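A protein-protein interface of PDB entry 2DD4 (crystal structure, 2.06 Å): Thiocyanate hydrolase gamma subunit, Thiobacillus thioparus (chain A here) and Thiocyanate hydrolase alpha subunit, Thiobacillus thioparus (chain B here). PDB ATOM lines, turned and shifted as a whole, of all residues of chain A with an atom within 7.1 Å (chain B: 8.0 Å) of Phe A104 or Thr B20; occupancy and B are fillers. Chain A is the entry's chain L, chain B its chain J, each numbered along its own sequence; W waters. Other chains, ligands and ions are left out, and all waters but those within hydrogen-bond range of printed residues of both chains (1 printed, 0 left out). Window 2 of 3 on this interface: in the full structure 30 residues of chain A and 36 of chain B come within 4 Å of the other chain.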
ATOM      1  N   TRP A  96       2.098   3.178 -18.976  1.00  0.00           N
ATOM      2  CA  TRP A  96       1.156   2.715 -17.971  1.00  0.00           C
ATOM      3  C   TRP A  96       0.066   3.707 -17.590  1.00  0.00           C
ATOM      4  O   TRP A  96      -0.993   3.309 -17.104  1.00  0.00           O
ATOM      5  CB  TRP A  96       1.918   2.236 -16.737  1.00  0.00           C
ATOM      6  CG  TRP A  96       2.580   0.918 -16.990  1.00  0.00           C
ATOM      7  CD1 TRP A  96       3.549   0.652 -17.916  1.00  0.00           C
ATOM      8  CD2 TRP A  96       2.265  -0.335 -16.368  1.00  0.00           C
ATOM      9  NE1 TRP A  96       3.851  -0.691 -17.915  1.00  0.00           N
ATOM     10  CE2 TRP A  96       3.078  -1.319 -16.974  1.00  0.00           C
ATOM     11  CE3 TRP A  96       1.372  -0.722 -15.359  1.00  0.00           C
ATOM     12  CZ2 TRP A  96       3.025  -2.669 -16.603  1.00  0.00           C
ATOM     13  CZ3 TRP A  96       1.319  -2.063 -14.991  1.00  0.00           C
ATOM     14  CH2 TRP A  96       2.143  -3.019 -15.613  1.00  0.00           C
ATOM     15  N   VAL A  97       0.310   4.992 -17.832  1.00  0.00           N
ATOM     16  CA  VAL A  97      -0.678   6.011 -17.509  1.00  0.00           C
ATOM     17  C   VAL A  97      -1.586   6.356 -18.691  1.00  0.00           C
ATOM     18  O   VAL A  97      -2.816   6.339 -18.565  1.00  0.00           O
ATOM     19  CB  VAL A  97       0.000   7.323 -17.020  1.00  0.00           C
ATOM     20  CG1 VAL A  97      -1.060   8.393 -16.762  1.00  0.00           C
ATOM     21  CG2 VAL A  97       0.805   7.065 -15.752  1.00  0.00           C
ATOM     22  N   THR A  98      -0.985   6.648 -19.843  1.00  0.00           N
ATOM     23  CA  THR A  98      -1.757   7.052 -21.016  1.00  0.00           C
ATOM     24  C   THR A  98      -2.146   6.009 -22.064  1.00  0.00           C
ATOM     25  O   THR A  98      -2.953   6.306 -22.946  1.00  0.00           O
ATOM     26  CB  THR A  98      -1.052   8.215 -21.746  1.00  0.00           C
ATOM     27  OG1 THR A  98       0.261   7.804 -22.153  1.00  0.00           O
ATOM     28  CG2 THR A  98      -0.936   9.423 -20.820  1.00  0.00           C
ATOM     29  N   SER A  99      -1.586   4.805 -21.996  1.00  0.00           N
ATOM     30  CA  SER A  99      -1.946   3.781 -22.978  1.00  0.00           C
ATOM     31  C   SER A  99      -3.351   3.233 -22.725  1.00  0.00           C
ATOM     32  O   SER A  99      -4.108   2.998 -23.668  1.00  0.00           O
ATOM     33  CB  SER A  99      -0.927   2.637 -22.977  1.00  0.00           C
ATOM     34  OG  SER A  99       0.289   3.044 -23.585  1.00  0.00           O
ATOM     35  N   PRO A 100      -3.717   3.006 -21.451  1.00  0.00           N
ATOM     36  CA  PRO A 100      -5.062   2.490 -21.175  1.00  0.00           C
ATOM     37  C   PRO A 100      -6.129   3.540 -21.501  1.00  0.00           C
ATOM     38  O   PRO A 100      -5.873   4.745 -21.427  1.00  0.00           O
ATOM     39  CB  PRO A 100      -5.007   2.160 -19.681  1.00  0.00           C
ATOM     40  CG  PRO A 100      -3.556   1.784 -19.478  1.00  0.00           C
ATOM     41  CD  PRO A 100      -2.855   2.875 -20.261  1.00  0.00           C
ATOM     42  N   PRO A 101      -7.341   3.096 -21.864  1.00  0.00           N
ATOM     43  CA  PRO A 101      -8.455   3.990 -22.206  1.00  0.00           C
ATOM     44  C   PRO A 101      -8.754   5.069 -21.162  1.00  0.00           C
ATOM     45  O   PRO A 101      -9.199   6.165 -21.503  1.00  0.00           O
ATOM     46  CB  PRO A 101      -9.627   3.026 -22.373  1.00  0.00           C
ATOM     47  CG  PRO A 101      -8.968   1.791 -22.888  1.00  0.00           C
ATOM     48  CD  PRO A 101      -7.744   1.685 -22.009  1.00  0.00           C
ATOM     49  N   THR A 102      -8.504   4.750 -19.895  1.00  0.00           N
ATOM     50  CA  THR A 102      -8.761   5.664 -18.777  1.00  0.00           C
ATOM     51  C   THR A 102      -7.899   6.922 -18.756  1.00  0.00           C
ATOM     52  O   THR A 102      -8.322   7.970 -18.266  1.00  0.00           O
ATOM     53  CB  THR A 102      -8.513   4.970 -17.430  1.00  0.00           C
ATOM     54  OG1 THR A 102      -7.113   4.675 -17.312  1.00  0.00           O
ATOM     55  CG2 THR A 102      -9.315   3.676 -17.327  1.00  0.00           C
ATOM     56  N   GLN A 103      -6.683   6.796 -19.271  1.00  0.00           N
ATOM     57  CA  GLN A 103      -5.700   7.873 -19.273  1.00  0.00           C
ATOM     58  C   GLN A 103      -5.192   8.113 -17.847  1.00  0.00           C
ATOM     59  O   GLN A 103      -4.698   9.193 -17.527  1.00  0.00           O
ATOM     60  CB  GLN A 103      -6.255   9.181 -19.853  1.00  0.00           C
ATOM     61  CG  GLN A 103      -5.140  10.092 -20.405  1.00  0.00           C
ATOM     62  CD  GLN A 103      -5.625  11.484 -20.777  1.00  0.00           C
ATOM     63  OE1 GLN A 103      -6.730  11.650 -21.281  1.00  0.00           O
ATOM     64  NE2 GLN A 103      -4.787  12.488 -20.537  1.00  0.00           N
ATOM     65  N   PHE A 104      -5.347   7.108 -16.986  1.00  0.00           N
ATOM     66  CA  PHE A 104      -4.829   7.175 -15.619  1.00  0.00           C
ATOM     67  C   PHE A 104      -4.459   5.767 -15.161  1.00  0.00           C
ATOM     68  O   PHE A 104      -4.497   5.447 -13.975  1.00  0.00           O
ATOM     69  CB  PHE A 104      -5.813   7.858 -14.637  1.00  0.00           C
ATOM     70  CG  PHE A 104      -7.168   7.197 -14.507  1.00  0.00           C
ATOM     71  CD1 PHE A 104      -7.313   5.965 -13.875  1.00  0.00           C
ATOM     72  CD2 PHE A 104      -8.317   7.859 -14.945  1.00  0.00           C
ATOM     73  CE1 PHE A 104      -8.578   5.404 -13.673  1.00  0.00           C
ATOM     74  CE2 PHE A 104      -9.588   7.309 -14.750  1.00  0.00           C
ATOM     75  CZ  PHE A 104      -9.719   6.080 -14.111  1.00  0.00           C
ATOM     76  N   GLY A 105      -4.066   4.947 -16.135  1.00  0.00           N
ATOM     77  CA  GLY A 105      -3.697   3.567 -15.874  1.00  0.00           C
ATOM     78  C   GLY A 105      -4.953   2.732 -15.741  1.00  0.00           C
ATOM     79  O   GLY A 105      -6.026   3.278 -15.463  1.00  0.00           O
ATOM     80  N   THR A 106      -4.859   1.423 -15.958  1.00  0.00           N
ATOM     81  CA  THR A 106      -6.053   0.602 -15.804  1.00  0.00           C
ATOM     82  C   THR A 106      -6.454   0.703 -14.335  1.00  0.00           C
ATOM     83  O   THR A 106      -5.613   0.916 -13.461  1.00  0.00           O
ATOM     84  CB  THR A 106      -5.803  -0.885 -16.153  1.00  0.00           C
ATOM     85  OG1 THR A 106      -4.790  -1.416 -15.290  1.00  0.00           O
ATOM     86  CG2 THR A 106      -5.365  -1.029 -17.611  1.00  0.00           C
ATOM     87  N   PRO A 107      -7.750   0.571 -14.043  1.00  0.00           N
ATOM     88  CA  PRO A 107      -8.169   0.663 -12.645  1.00  0.00           C
ATOM     89  C   PRO A 107      -7.559  -0.418 -11.753  1.00  0.00           C
ATOM     90  O   PRO A 107      -7.256  -0.167 -10.585  1.00  0.00           O
ATOM     91  CB  PRO A 107      -9.685   0.542 -12.738  1.00  0.00           C
ATOM     92  CG  PRO A 107      -9.980   1.201 -14.052  1.00  0.00           C
ATOM     93  CD  PRO A 107      -8.915   0.615 -14.945  1.00  0.00           C
ATOM     94  N   TYR A 110      -2.924  -0.477 -12.116  1.00  0.00           N
ATOM     95  CA  TYR A 110      -2.241   0.724 -11.636  1.00  0.00           C
ATOM     96  C   TYR A 110      -1.061   1.155 -12.503  1.00  0.00           C
ATOM     97  O   TYR A 110      -0.910   0.696 -13.638  1.00  0.00           O
ATOM     98  CB  TYR A 110      -1.792   0.535 -10.183  1.00  0.00           C
ATOM     99  CG  TYR A 110      -2.938   0.181  -9.258  1.00  0.00           C
ATOM    100  CD1 TYR A 110      -3.075  -1.110  -8.752  1.00  0.00           C
ATOM    101  CD2 TYR A 110      -3.914   1.123  -8.932  1.00  0.00           C
ATOM    102  CE1 TYR A 110      -4.156  -1.458  -7.945  1.00  0.00           C
ATOM    103  CE2 TYR A 110      -5.005   0.785  -8.127  1.00  0.00           C
ATOM    104  CZ  TYR A 110      -5.115  -0.512  -7.639  1.00  0.00           C
ATOM    105  OH  TYR A 110      -6.181  -0.864  -6.847  1.00  0.00           O
ATOM    106  N   CYS A 111      -0.225   2.037 -11.962  1.00  0.00           N
ATOM    107  CA  CYS A 111       0.908   2.560 -12.715  1.00  0.00           C
ATOM    108  C   CYS A 111       2.253   2.458 -12.001  1.00  0.00           C
ATOM    109  O   CYS A 111       2.994   3.438 -11.930  1.00  0.00           O
ATOM    110  CB  CYS A 111       0.640   4.023 -13.073  1.00  0.00           C
ATOM    111  SG  CYS A 111      -1.040   4.329 -13.661  1.00  0.00           S
ATOM    112  N   THR B  13     -16.922  11.042 -10.257  1.00  0.00           N
ATOM    113  CA  THR B  13     -15.937  11.748 -11.075  1.00  0.00           C
ATOM    114  C   THR B  13     -14.663  12.090 -10.314  1.00  0.00           C
ATOM    115  O   THR B  13     -13.661  12.461 -10.918  1.00  0.00           O
ATOM    116  CB  THR B  13     -16.499  13.072 -11.641  1.00  0.00           C
ATOM    117  OG1 THR B  13     -16.726  13.992 -10.566  1.00  0.00           O
ATOM    118  CG2 THR B  13     -17.798  12.829 -12.395  1.00  0.00           C
ATOM    119  N   HIS B  14     -14.698  11.965  -8.992  1.00  0.00           N
ATOM    120  CA  HIS B  14     -13.540  12.297  -8.172  1.00  0.00           C
ATOM    121  C   HIS B  14     -12.226  11.621  -8.562  1.00  0.00           C
ATOM    122  O   HIS B  14     -11.216  12.294  -8.776  1.00  0.00           O
ATOM    123  CB  HIS B  14     -13.806  11.990  -6.701  1.00  0.00           C
ATOM    124  CG  HIS B  14     -12.586  12.124  -5.845  1.00  0.00           C
ATOM    125  ND1 HIS B  14     -11.984  13.339  -5.598  1.00  0.00           N
ATOM    126  CD2 HIS B  14     -11.807  11.190  -5.250  1.00  0.00           C
ATOM    127  CE1 HIS B  14     -10.885  13.148  -4.891  1.00  0.00           C
ATOM    128  NE2 HIS B  14     -10.754  11.853  -4.667  1.00  0.00           N
ATOM    129  N   HIS B  15     -12.231  10.295  -8.633  1.00  0.00           N
ATOM    130  CA  HIS B  15     -11.012   9.564  -8.966  1.00  0.00           C
ATOM    131  C   HIS B  15     -10.422   9.976 -10.311  1.00  0.00           C
ATOM    132  O   HIS B  15      -9.223  10.225 -10.417  1.00  0.00           O
ATOM    133  CB  HIS B  15     -11.268   8.054  -8.964  1.00  0.00           C
ATOM    134  CG  HIS B  15     -10.025   7.235  -9.122  1.00  0.00           C
ATOM    135  ND1 HIS B  15      -9.023   7.218  -8.176  1.00  0.00           N
ATOM    136  CD2 HIS B  15      -9.608   6.430 -10.127  1.00  0.00           C
ATOM    137  CE1 HIS B  15      -8.041   6.438  -8.592  1.00  0.00           C
ATOM    138  NE2 HIS B  15      -8.371   5.948  -9.773  1.00  0.00           N
ATOM    139  N   ALA B  16     -11.262  10.048 -11.336  1.00  0.00           N
ATOM    140  CA  ALA B  16     -10.795  10.421 -12.665  1.00  0.00           C
ATOM    141  C   ALA B  16     -10.212  11.834 -12.701  1.00  0.00           C
ATOM    142  O   ALA B  16      -9.151  12.059 -13.287  1.00  0.00           O
ATOM    143  CB  ALA B  16     -11.932  10.298 -13.671  1.00  0.00           C
ATOM    144  N   LYS B  17     -10.902  12.787 -12.081  1.00  0.00           N
ATOM    145  CA  LYS B  17     -10.423  14.165 -12.076  1.00  0.00           C
ATOM    146  C   LYS B  17      -9.054  14.249 -11.427  1.00  0.00           C
ATOM    147  O   LYS B  17      -8.189  15.007 -11.861  1.00  0.00           O
ATOM    148  CB  LYS B  17     -11.397  15.072 -11.323  1.00  0.00           C
ATOM    149  CG  LYS B  17     -12.720  15.281 -12.035  1.00  0.00           C
ATOM    150  CD  LYS B  17     -13.673  16.115 -11.202  1.00  0.00           C
ATOM    151  CE  LYS B  17     -14.989  16.325 -11.937  1.00  0.00           C
ATOM    152  NZ  LYS B  17     -16.025  16.955 -11.070  1.00  0.00           N
ATOM    153  N   MET B  18      -8.861  13.448 -10.388  1.00  0.00           N
ATOM    154  CA  MET B  18      -7.607  13.438  -9.654  1.00  0.00           C
ATOM    155  C   MET B  18      -6.458  12.691 -10.327  1.00  0.00           C
ATOM    156  O   MET B  18      -5.312  13.131 -10.268  1.00  0.00           O
ATOM    157  CB  MET B  18      -7.847  12.844  -8.265  1.00  0.00           C
ATOM    158  CG  MET B  18      -6.587  12.508  -7.499  1.00  0.00           C
ATOM    159  SD  MET B  18      -6.966  11.791  -5.892  1.00  0.00           S
ATOM    160  CE  MET B  18      -7.433  10.111  -6.374  1.00  0.00           C
ATOM    161  N   ALA B  19      -6.757  11.572 -10.980  1.00  0.00           N
ATOM    162  CA  ALA B  19      -5.693  10.772 -11.582  1.00  0.00           C
ATOM    163  C   ALA B  19      -5.442  10.909 -13.080  1.00  0.00           C
ATOM    164  O   ALA B  19      -4.387  10.505 -13.562  1.00  0.00           O
ATOM    165  CB  ALA B  19      -5.915   9.297 -11.235  1.00  0.00           C
ATOM    166  N   THR B  20      -6.392  11.465 -13.820  1.00  0.00           N
ATOM    167  CA  THR B  20      -6.216  11.592 -15.263  1.00  0.00           C
ATOM    168  C   THR B  20      -4.930  12.319 -15.646  1.00  0.00           C
ATOM    169  O   THR B  20      -4.628  13.399 -15.135  1.00  0.00           O
ATOM    170  CB  THR B  20      -7.431  12.289 -15.904  1.00  0.00           C
ATOM    171  OG1 THR B  20      -8.591  11.468 -15.714  1.00  0.00           O
ATOM    172  CG2 THR B  20      -7.214  12.502 -17.400  1.00  0.00           C
ATOM    173  N   GLY B  21      -4.163  11.696 -16.537  1.00  0.00           N
ATOM    174  CA  GLY B  21      -2.916  12.283 -16.996  1.00  0.00           C
ATOM    175  C   GLY B  21      -1.788  12.210 -15.986  1.00  0.00           C
ATOM    176  O   GLY B  21      -0.678  12.658 -16.265  1.00  0.00           O
ATOM    177  N   ILE B  22      -2.065  11.642 -14.815  1.00  0.00           N
ATOM    178  CA  ILE B  22      -1.063  11.526 -13.763  1.00  0.00           C
ATOM    179  C   ILE B  22      -0.835  10.065 -13.375  1.00  0.00           C
ATOM    180  O   ILE B  22       0.301   9.593 -13.323  1.00  0.00           O
ATOM    181  CB  ILE B  22      -1.493  12.315 -12.505  1.00  0.00           C
ATOM    182  CG1 ILE B  22      -1.657  13.795 -12.852  1.00  0.00           C
ATOM    183  CG2 ILE B  22      -0.464  12.142 -11.398  1.00  0.00           C
ATOM    184  CD1 ILE B  22      -2.154  14.646 -11.693  1.00  0.00           C
ATOM    185  N   GLY B  23      -1.923   9.359 -13.094  1.00  0.00           N
ATOM    186  CA  GLY B  23      -1.818   7.961 -12.721  1.00  0.00           C
ATOM    187  C   GLY B  23      -2.055   7.679 -11.247  1.00  0.00           C
ATOM    188  O   GLY B  23      -2.129   8.587 -10.421  1.00  0.00           O
ATOM    189  N   ASP B  24      -2.165   6.395 -10.930  1.00  0.00           N
ATOM    190  CA  ASP B  24      -2.389   5.910  -9.572  1.00  0.00           C
ATOM    191  C   ASP B  24      -1.273   4.880  -9.399  1.00  0.00           C
ATOM    192  O   ASP B  24      -1.166   3.955 -10.201  1.00  0.00           O
ATOM    193  CB  ASP B  24      -3.767   5.235  -9.511  1.00  0.00           C
ATOM    194  CG  ASP B  24      -4.133   4.728  -8.123  1.00  0.00           C
ATOM    195  OD1 ASP B  24      -3.293   4.786  -7.203  1.00  0.00           O
ATOM    196  OD2 ASP B  24      -5.281   4.258  -7.962  1.00  0.00           O
ATOM    197  N   PRO B  25      -0.469   4.981  -8.327  1.00  0.00           N
ATOM    198  CA  PRO B  25      -0.462   5.939  -7.215  1.00  0.00           C
ATOM    199  C   PRO B  25       0.244   7.289  -7.384  1.00  0.00           C
ATOM    200  O   PRO B  25       0.402   8.018  -6.403  1.00  0.00           O
ATOM    201  CB  PRO B  25       0.170   5.127  -6.096  1.00  0.00           C
ATOM    202  CG  PRO B  25       1.263   4.416  -6.830  1.00  0.00           C
ATOM    203  CD  PRO B  25       0.585   3.965  -8.130  1.00  0.00           C
ATOM    204  N   GLN B  26       0.676   7.629  -8.596  1.00  0.00           N
ATOM    205  CA  GLN B  26       1.356   8.905  -8.801  1.00  0.00           C
ATOM    206  C   GLN B  26       0.557  10.096  -8.269  1.00  0.00           C
ATOM    207  O   GLN B  26       1.131  11.068  -7.786  1.00  0.00           O
ATOM    208  CB  GLN B  26       1.666   9.132 -10.291  1.00  0.00           C
ATOM    209  CG  GLN B  26       2.805   8.272 -10.845  1.00  0.00           C
ATOM    210  CD  GLN B  26       2.332   6.911 -11.323  1.00  0.00           C
ATOM    211  OE1 GLN B  26       1.286   6.423 -10.896  1.00  0.00           O
ATOM    212  NE2 GLN B  26       3.107   6.287 -12.205  1.00  0.00           N
ATOM    213  N   CYS B  27      -0.768  10.015  -8.344  1.00  0.00           N
ATOM    214  CA  CYS B  27      -1.622  11.109  -7.887  1.00  0.00           C
ATOM    215  C   CYS B  27      -1.595  11.366  -6.376  1.00  0.00           C
ATOM    216  O   CYS B  27      -2.114  12.377  -5.918  1.00  0.00           O
ATOM    217  CB  CYS B  27      -3.067  10.874  -8.343  1.00  0.00           C
ATOM    218  SG  CYS B  27      -3.819   9.345  -7.724  1.00  0.00           S
HETATM  219  O   HOH W   1       4.149   4.968  -9.486  1.00  0.00           O
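The backbone carbonyl oxygen of Gln A103 lies within hydrogen-bond range of the backbone NH of Gly B21 (2.7 Å). N of Cys A111 lies within hydrogen-bond range of O of Asp B24, 2.8 Å away. The side-chain amide nitrogen (NE2) of Gln B26 sits at hydrogen-bond distance from the backbone carbonyl oxygen (O) of Cys A111.
The side-chain hydroxyl (OG1) of Thr B20 is in hydrogen-bond range of the backbone carbonyl oxygen (O) of Ala B16. The backbone carbonyl oxygen of Gly B23 sits close to the side-chain sulfur of Cys B27 (3.3 Å). N of Asp B24 lies close to OE1 of Gln B26 (3.5 Å). The backbone NH of Phe A104 is in hydrogen-bond range of the backbone carbonyl oxygen of Val A97. The backbone carbonyl oxygen (O) of Val A97 sits at hydrogen-bond distance from the backbone NH (N) of Gly A105 (3.1 Å). OG1 of Thr A102 is in hydrogen-bond range of N of Phe A104 (3.0 Å).
Gly B21 touches Val A97 (C to CG1, 3.96 Å). Val A97 touches Ile B22 (CG2 to O, 3.5 Å). Gly B23 touches Val A97 (N to CG1, 3.9 Å). His B15 touches Phe A104 (CD2 to CE1, 3.8 Å). Ala B16 touches Phe A104 (CA to CE2, 3.9 Å). CD2 of Phe A104 touches OG1 of Thr B20, at 3.7 Å. Phe A104 touches Gly B23. Phe A104 touches Asp B24. Asp B24 touches Tyr A110. Cys A111 touches Gly B23 (SG to CA, 3.8 Å).
Printed residues of chain B within 4 Å of Val A97: Gly B21, Ile B22 and Gly B23. Of chain B, only His B15 (3.8 Å), Ala B16 (3.9 Å), Ala B19 (3.2 Å), Thr B20 (3.7 Å), Gly B23 (3.9 Å) and Asp B24 (3.95 Å) come within 4 Å of Phe A104. No residue of chain B comes within 4 Å of Gly A105. Of the printed residues of chain B, Tyr A110 touches Asp B24 (3.5 Å). Printed residues of chain A within 4 Å of His B15: Phe A104 (3.8 Å). Lys B17 touches none of the printed residues of chain A. Of the printed residues of chain A, Thr B20 touches Gln A103 and Phe A104. Of the printed residues of chain A, Gly B23 touches Val A97, Phe A104 and Cys A111. Printed residues of chain A within 4 Å of Gln B26: Cys A111 (2.9 Å). The nearest printed residue of chain A that does not touch Asp B24 is Pro A107 (5.5 Å).
Of the 15 printed residues of chain B, 9 touch a printed residue of chain A. Hydrophobic or aromatic side chains of chain B that line the printed part of chain A: His B15, Ala B16 and Ala B19. Printed residues of chain A that touch a printed residue of chain B: Val A97, Gln A103, Phe A104, Tyr A110 and Cys A111. Hydrophobic or aromatic side chains of chain A within 4 Å of the printed part of chain B: Val A97, Phe A104 and Tyr A110. Among the printed residues, 15 pairs touch across the chains. Among the printed residues, no Asp or Glu carboxylate lies within 4 Å of a Lys or Arg side-chain nitrogen of the other chain.
Water W1 bridges O of Cys A111 (3.1 Å) and NE2 of Gln B26 (3.2 Å).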
